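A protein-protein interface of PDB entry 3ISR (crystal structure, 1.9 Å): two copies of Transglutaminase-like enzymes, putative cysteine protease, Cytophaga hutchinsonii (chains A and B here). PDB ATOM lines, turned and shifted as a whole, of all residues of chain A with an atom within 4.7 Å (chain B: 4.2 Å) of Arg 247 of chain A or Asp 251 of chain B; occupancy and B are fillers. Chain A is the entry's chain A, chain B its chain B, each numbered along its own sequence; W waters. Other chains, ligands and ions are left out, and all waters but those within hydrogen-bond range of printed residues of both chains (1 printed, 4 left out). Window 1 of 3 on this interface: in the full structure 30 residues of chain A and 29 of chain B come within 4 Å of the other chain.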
ATOM      1  N   PRO A 115     -14.431  -0.081  -2.493  1.00  0.00           N
ATOM      2  CA  PRO A 115     -13.010  -0.044  -2.216  1.00  0.00           C
ATOM      3  C   PRO A 115     -12.561   1.283  -1.577  1.00  0.00           C
ATOM      4  O   PRO A 115     -11.558   1.300  -0.878  1.00  0.00           O
ATOM      5  CB  PRO A 115     -12.379  -0.175  -3.609  1.00  0.00           C
ATOM      6  CG  PRO A 115     -13.395  -0.934  -4.393  1.00  0.00           C
ATOM      7  CD  PRO A 115     -14.702  -0.407  -3.913  1.00  0.00           C
ATOM      8  N   PHE A 116     -13.297   2.369  -1.823  1.00  0.00           N
ATOM      9  CA  PHE A 116     -12.906   3.693  -1.301  1.00  0.00           C
ATOM     10  C   PHE A 116     -13.319   3.912   0.142  1.00  0.00           C
ATOM     11  O   PHE A 116     -13.101   4.974   0.685  1.00  0.00           O
ATOM     12  CB  PHE A 116     -13.377   4.809  -2.246  1.00  0.00           C
ATOM     13  CG  PHE A 116     -12.840   4.638  -3.619  1.00  0.00           C
ATOM     14  CD1 PHE A 116     -11.543   5.042  -3.917  1.00  0.00           C
ATOM     15  CD2 PHE A 116     -13.594   4.005  -4.608  1.00  0.00           C
ATOM     16  CE1 PHE A 116     -11.002   4.855  -5.192  1.00  0.00           C
ATOM     17  CE2 PHE A 116     -13.055   3.811  -5.906  1.00  0.00           C
ATOM     18  CZ  PHE A 116     -11.758   4.245  -6.189  1.00  0.00           C
ATOM     19  N   PHE A 118     -11.866   1.713   2.250  1.00  0.00           N
ATOM     20  CA  PHE A 118     -10.768   0.990   2.918  1.00  0.00           C
ATOM     21  C   PHE A 118      -9.460   1.767   3.044  1.00  0.00           C
ATOM     22  O   PHE A 118      -9.164   2.652   2.234  1.00  0.00           O
ATOM     23  CB  PHE A 118     -10.538  -0.379   2.244  1.00  0.00           C
ATOM     24  CG  PHE A 118     -11.679  -1.341   2.476  1.00  0.00           C
ATOM     25  CD1 PHE A 118     -11.696  -2.171   3.591  1.00  0.00           C
ATOM     26  CD2 PHE A 118     -12.758  -1.372   1.606  1.00  0.00           C
ATOM     27  CE1 PHE A 118     -12.774  -3.044   3.815  1.00  0.00           C
ATOM     28  CE2 PHE A 118     -13.830  -2.226   1.818  1.00  0.00           C
ATOM     29  CZ  PHE A 118     -13.843  -3.057   2.923  1.00  0.00           C
ATOM     30  N   PRO A 119      -8.662   1.429   4.060  1.00  0.00           N
ATOM     31  CA  PRO A 119      -7.364   2.091   4.222  1.00  0.00           C
ATOM     32  C   PRO A 119      -6.493   1.837   2.997  1.00  0.00           C
ATOM     33  O   PRO A 119      -6.622   0.789   2.342  1.00  0.00           O
ATOM     34  CB  PRO A 119      -6.746   1.381   5.440  1.00  0.00           C
ATOM     35  CG  PRO A 119      -7.849   0.621   6.104  1.00  0.00           C
ATOM     36  CD  PRO A 119      -8.871   0.330   5.032  1.00  0.00           C
ATOM     37  N   SER A 120      -5.613   2.781   2.689  1.00  0.00           N
ATOM     38  CA  SER A 120      -4.647   2.584   1.613  1.00  0.00           C
ATOM     39  C   SER A 120      -3.253   2.975   2.117  1.00  0.00           C
ATOM     40  O   SER A 120      -3.104   3.369   3.281  1.00  0.00           O
ATOM     41  CB  SER A 120      -5.066   3.399   0.388  1.00  0.00           C
ATOM     42  OG  SER A 120      -5.125   4.780   0.704  1.00  0.00           O
ATOM     43  N   CYS A 123      -3.188   6.453   3.553  1.00  0.00           N
ATOM     44  CA  CYS A 123      -4.443   6.833   4.228  1.00  0.00           C
ATOM     45  C   CYS A 123      -4.841   5.723   5.192  1.00  0.00           C
ATOM     46  O   CYS A 123      -5.714   4.916   4.895  1.00  0.00           O
ATOM     47  CB  CYS A 123      -5.592   7.080   3.199  1.00  0.00           C
ATOM     48  SG  CYS A 123      -5.136   8.264   1.910  1.00  0.00           S
ATOM     49  N   ILE A 189      -8.784  12.356   2.984  1.00  0.00           N
ATOM     50  CA  ILE A 189      -9.288  11.013   2.615  1.00  0.00           C
ATOM     51  C   ILE A 189      -9.318  10.064   3.826  1.00  0.00           C
ATOM     52  O   ILE A 189     -10.313   9.357   4.066  1.00  0.00           O
ATOM     53  CB  ILE A 189      -8.409  10.421   1.508  1.00  0.00           C
ATOM     54  CG1 ILE A 189      -8.615  11.194   0.193  1.00  0.00           C
ATOM     55  CG2 ILE A 189      -8.712   8.904   1.272  1.00  0.00           C
ATOM     56  CD1 ILE A 189      -7.552  10.852  -0.874  1.00  0.00           C
ATOM     57  N   ARG A 193     -12.728   8.264   5.378  1.00  0.00           N
ATOM     58  CA  ARG A 193     -12.872   6.805   5.489  1.00  0.00           C
ATOM     59  C   ARG A 193     -13.010   6.394   6.931  1.00  0.00           C
ATOM     60  O   ARG A 193     -13.746   5.451   7.244  1.00  0.00           O
ATOM     61  CB  ARG A 193     -11.694   6.070   4.829  1.00  0.00           C
ATOM     62  CG  ARG A 193     -11.599   6.336   3.316  1.00  0.00           C
ATOM     63  CD  ARG A 193     -10.515   5.441   2.656  1.00  0.00           C
ATOM     64  NE  ARG A 193     -10.301   5.822   1.265  1.00  0.00           N
ATOM     65  CZ  ARG A 193      -9.155   5.720   0.601  1.00  0.00           C
ATOM     66  NH1 ARG A 193      -8.061   5.270   1.195  1.00  0.00           N
ATOM     67  NH2 ARG A 193      -9.097   6.141  -0.645  1.00  0.00           N
ATOM     68  N   TYR A 201      -8.608   9.986  -4.013  1.00  0.00           N
ATOM     69  CA  TYR A 201      -7.569  10.977  -4.367  1.00  0.00           C
ATOM     70  C   TYR A 201      -7.829  11.504  -5.756  1.00  0.00           C
ATOM     71  O   TYR A 201      -8.192  10.734  -6.637  1.00  0.00           O
ATOM     72  CB  TYR A 201      -6.263  10.192  -4.424  1.00  0.00           C
ATOM     73  CG  TYR A 201      -4.969  11.000  -4.454  1.00  0.00           C
ATOM     74  CD1 TYR A 201      -4.544  11.688  -3.331  1.00  0.00           C
ATOM     75  CD2 TYR A 201      -4.137  10.978  -5.576  1.00  0.00           C
ATOM     76  CE1 TYR A 201      -3.325  12.407  -3.330  1.00  0.00           C
ATOM     77  CE2 TYR A 201      -2.911  11.701  -5.586  1.00  0.00           C
ATOM     78  CZ  TYR A 201      -2.535  12.401  -4.447  1.00  0.00           C
ATOM     79  OH  TYR A 201      -1.349  13.104  -4.369  1.00  0.00           O
ATOM     80  N   GLY A 246      -7.905   7.883  -7.752  1.00  0.00           N
ATOM     81  CA  GLY A 246      -7.448   6.581  -7.265  1.00  0.00           C
ATOM     82  C   GLY A 246      -7.585   6.544  -5.756  1.00  0.00           C
ATOM     83  O   GLY A 246      -8.186   7.426  -5.159  1.00  0.00           O
ATOM     84  N   ARG A 247      -7.050   5.507  -5.136  1.00  0.00           N
ATOM     85  CA  ARG A 247      -7.222   5.348  -3.689  1.00  0.00           C
ATOM     86  C   ARG A 247      -6.341   6.367  -2.955  1.00  0.00           C
ATOM     87  O   ARG A 247      -6.739   6.912  -1.917  1.00  0.00           O
ATOM     88  CB  ARG A 247      -6.909   3.906  -3.274  1.00  0.00           C
ATOM     89  CG  ARG A 247      -7.873   2.906  -3.923  1.00  0.00           C
ATOM     90  CD  ARG A 247      -7.535   1.431  -3.628  1.00  0.00           C
ATOM     91  NE  ARG A 247      -7.482   1.149  -2.196  1.00  0.00           N
ATOM     92  CZ  ARG A 247      -7.250  -0.054  -1.656  1.00  0.00           C
ATOM     93  NH1 ARG A 247      -7.212  -0.177  -0.329  1.00  0.00           N
ATOM     94  NH2 ARG A 247      -7.029  -1.128  -2.429  1.00  0.00           N
ATOM     95  N   ASP A 248      -5.156   6.601  -3.505  1.00  0.00           N
ATOM     96  CA  ASP A 248      -4.224   7.611  -2.984  1.00  0.00           C
ATOM     97  C   ASP A 248      -3.128   7.792  -4.023  1.00  0.00           C
ATOM     98  O   ASP A 248      -3.249   7.242  -5.114  1.00  0.00           O
ATOM     99  CB  ASP A 248      -3.666   7.267  -1.573  1.00  0.00           C
ATOM    100  CG  ASP A 248      -2.882   5.954  -1.512  1.00  0.00           C
ATOM    101  OD1 ASP A 248      -2.337   5.517  -2.530  1.00  0.00           O
ATOM    102  OD2 ASP A 248      -2.757   5.382  -0.386  1.00  0.00           O
ATOM    103  N   ASP A 251      -1.568   5.322  -6.637  1.00  0.00           N
ATOM    104  CA  ASP A 251      -2.297   5.054  -7.880  1.00  0.00           C
ATOM    105  C   ASP A 251      -2.193   6.200  -8.896  1.00  0.00           C
ATOM    106  O   ASP A 251      -2.803   6.134  -9.967  1.00  0.00           O
ATOM    107  CB  ASP A 251      -3.783   4.837  -7.594  1.00  0.00           C
ATOM    108  CG  ASP A 251      -4.066   3.534  -6.887  1.00  0.00           C
ATOM    109  OD1 ASP A 251      -3.273   2.577  -7.032  1.00  0.00           O
ATOM    110  OD2 ASP A 251      -5.106   3.460  -6.193  1.00  0.00           O
ATOM    111  N   PHE B  69     -17.510 -11.124  -2.821  1.00  0.00           N
ATOM    112  CA  PHE B  69     -17.926 -10.600  -1.528  1.00  0.00           C
ATOM    113  C   PHE B  69     -19.405 -10.869  -1.296  1.00  0.00           C
ATOM    114  O   PHE B  69     -20.171 -10.929  -2.248  1.00  0.00           O
ATOM    115  CB  PHE B  69     -17.661  -9.096  -1.477  1.00  0.00           C
ATOM    116  CG  PHE B  69     -16.197  -8.731  -1.543  1.00  0.00           C
ATOM    117  CD1 PHE B  69     -15.349  -9.011  -0.469  1.00  0.00           C
ATOM    118  CD2 PHE B  69     -15.678  -8.090  -2.665  1.00  0.00           C
ATOM    119  CE1 PHE B  69     -13.983  -8.669  -0.502  1.00  0.00           C
ATOM    120  CE2 PHE B  69     -14.319  -7.724  -2.728  1.00  0.00           C
ATOM    121  CZ  PHE B  69     -13.457  -8.016  -1.632  1.00  0.00           C
ATOM    122  N   GLY B 246      -5.474  -9.775  -4.119  1.00  0.00           N
ATOM    123  CA  GLY B 246      -5.576  -8.324  -4.219  1.00  0.00           C
ATOM    124  C   GLY B 246      -4.239  -7.740  -3.794  1.00  0.00           C
ATOM    125  O   GLY B 246      -3.267  -8.463  -3.623  1.00  0.00           O
ATOM    126  N   ARG B 247      -4.201  -6.432  -3.611  1.00  0.00           N
ATOM    127  CA  ARG B 247      -2.953  -5.766  -3.274  1.00  0.00           C
ATOM    128  C   ARG B 247      -2.458  -6.184  -1.889  1.00  0.00           C
ATOM    129  O   ARG B 247      -1.262  -6.384  -1.690  1.00  0.00           O
ATOM    130  CB  ARG B 247      -3.135  -4.247  -3.380  1.00  0.00           C
ATOM    131  CG  ARG B 247      -3.439  -3.796  -4.781  1.00  0.00           C
ATOM    132  CD  ARG B 247      -3.768  -2.293  -4.872  1.00  0.00           C
ATOM    133  NE  ARG B 247      -2.596  -1.479  -4.529  1.00  0.00           N
ATOM    134  CZ  ARG B 247      -2.560  -0.146  -4.539  1.00  0.00           C
ATOM    135  NH1 ARG B 247      -1.443   0.474  -4.189  1.00  0.00           N
ATOM    136  NH2 ARG B 247      -3.634   0.559  -4.899  1.00  0.00           N
ATOM    137  N   ASP B 248      -3.383  -6.326  -0.945  1.00  0.00           N
ATOM    138  CA  ASP B 248      -3.070  -6.775   0.411  1.00  0.00           C
ATOM    139  C   ASP B 248      -4.387  -7.061   1.085  1.00  0.00           C
ATOM    140  O   ASP B 248      -5.420  -7.073   0.399  1.00  0.00           O
ATOM    141  CB  ASP B 248      -2.217  -5.756   1.203  1.00  0.00           C
ATOM    142  CG  ASP B 248      -2.870  -4.393   1.378  1.00  0.00           C
ATOM    143  OD1 ASP B 248      -4.099  -4.248   1.299  1.00  0.00           O
ATOM    144  OD2 ASP B 248      -2.107  -3.415   1.624  1.00  0.00           O
ATOM    145  N   ALA B 249      -4.361  -7.281   2.394  1.00  0.00           N
ATOM    146  CA  ALA B 249      -5.584  -7.700   3.131  1.00  0.00           C
ATOM    147  C   ALA B 249      -6.711  -6.658   3.098  1.00  0.00           C
ATOM    148  O   ALA B 249      -7.857  -7.010   3.315  1.00  0.00           O
ATOM    149  CB  ALA B 249      -5.259  -8.089   4.565  1.00  0.00           C
ATOM    150  N   ALA B 250      -6.410  -5.392   2.790  1.00  0.00           N
ATOM    151  CA  ALA B 250      -7.479  -4.394   2.685  1.00  0.00           C
ATOM    152  C   ALA B 250      -8.460  -4.802   1.580  1.00  0.00           C
ATOM    153  O   ALA B 250      -9.644  -4.418   1.602  1.00  0.00           O
ATOM    154  CB  ALA B 250      -6.897  -2.992   2.386  1.00  0.00           C
ATOM    155  N   ASP B 251      -7.961  -5.549   0.594  1.00  0.00           N
ATOM    156  CA  ASP B 251      -8.794  -5.991  -0.535  1.00  0.00           C
ATOM    157  C   ASP B 251      -9.321  -7.412  -0.366  1.00  0.00           C
ATOM    158  O   ASP B 251      -9.955  -7.953  -1.287  1.00  0.00           O
ATOM    159  CB  ASP B 251      -7.979  -5.997  -1.823  1.00  0.00           C
ATOM    160  CG  ASP B 251      -7.552  -4.623  -2.269  1.00  0.00           C
ATOM    161  OD1 ASP B 251      -8.258  -3.622  -1.993  1.00  0.00           O
ATOM    162  OD2 ASP B 251      -6.520  -4.571  -2.964  1.00  0.00           O
ATOM    163  N   ALA B 252      -9.033  -8.045   0.762  1.00  0.00           N
ATOM    164  CA  ALA B 252      -9.401  -9.459   0.930  1.00  0.00           C
ATOM    165  C   ALA B 252      -9.600  -9.854   2.383  1.00  0.00           C
ATOM    166  O   ALA B 252      -9.147 -10.929   2.806  1.00  0.00           O
ATOM    167  CB  ALA B 252      -8.339 -10.362   0.289  1.00  0.00           C
ATOM    168  N   ALA B 253     -10.280  -9.009   3.151  1.00  0.00           N
ATOM    169  CA  ALA B 253     -10.552  -9.343   4.560  1.00  0.00           C
ATOM    170  C   ALA B 253     -11.560 -10.473   4.647  1.00  0.00           C
ATOM    171  O   ALA B 253     -12.467 -10.558   3.815  1.00  0.00           O
ATOM    172  CB  ALA B 253     -11.085  -8.136   5.303  1.00  0.00           C
HETATM  173  O   HOH W   1      -6.540  -0.760  -5.873  1.00  0.00           O
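Arg 247 of chain A touches Asp 251 of chain B, and with the chains exchanged Asp 251 of chain A touches Arg 247 of chain B. 4 positions are printed for both chains. Of the 5 pairs that touch across the chains among the printed residues, 2 have their exchanged pair printed and touching as well.
Phe 116 of chain A touches none of the printed residues of chain B. Printed residues of chain B within 4 Å of Phe 118 of chain A: Ala 250. Printed residues of chain B within 4 Å of Pro 119 of chain A: Ala 250 (3.8 Å). Arg 247 of chain A touches just these residues of chain B: Ala 250 (3.9 Å) and Asp 251 (2.8 Å). Of the printed residues of chain B, Asp 251 of chain A touches Arg 247. Of the printed residues of chain A, Arg 247 of chain B touches Asp 251. Printed residues of chain A within 4 Å of Ala 250 of chain B: Phe 118, Pro 119 and Arg 247. The nearest printed residue of chain B that does not touch Arg 247 of chain A is Arg 247 of chain B (4.2 Å). The nearest printed residue of chain A that does not touch Asp 251 of chain B is Pro 115 of chain A (5.6 Å). The nearest printed residue of chain A that does not touch Arg 247 of chain B is Arg 247 of chain A (4.2 Å).
Water W1 lies within hydrogen-bond range of NH2 of Arg 247 of chain B (3.3 Å) and NH2 of Arg 247 of chain A (3.5 Å).
Of the 13 printed residues of chain A, 4 touch a printed residue of chain B. Of the 9 printed residues of chain B, 3 touch a printed residue of chain A. Among the printed residues, Asp or Glu carboxylates within 4 Å of a Lys or Arg side-chain nitrogen of the other chain: Arg 247 of chain A with Asp 251 of chain B (2.8 Å) and Asp 251 of chain A with Arg 247 of chain B (3.0 Å).
The backbone NH (N) of Arg 247 of chain A lies within hydrogen-bond range of the side-chain carboxylate (OD2) of Asp 251 of chain A, 3.0 Å away. O of Phe 118 of chain A sits at hydrogen-bond distance from NH1 of Arg 193 of chain A (3.0 Å). The side-chain carboxylate (OD1) of Asp 248 of chain B lies within hydrogen-bond range of the backbone NH (N) of Ala 250 of chain B (3.0 Å). NH2 of Arg 193 of chain A is in hydrogen-bond range of O of Arg 247 of chain A (2.8 Å). The guanidinium group of Arg 247 of chain A sits at hydrogen-bond distance from the backbone carbonyl oxygen of Pro 119 of chain A, 2.9 Å away. The backbone NH (N) of Arg 247 of chain B is in hydrogen-bond range of the side-chain carboxylate (OD2) of Asp 251 of chain B, at 3.0 Å.
CD1 of Phe 118 of chain A touches O of Ala 250 of chain B, 3.6 Å away. O of Pro 119 of chain A touches CB of Ala 250 of chain B (3.8 Å). Arg 247 of chain A touches Ala 250 of chain B.
The guanidinium group of Arg 247 of chain A lies within salt-bridge range of the side-chain carboxylate of Asp 251 of chain B (2.8 Å). NH2 of Arg 247 of chain B lies within salt-bridge range of OD1 of Asp 251 of chain A (3.0 Å).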
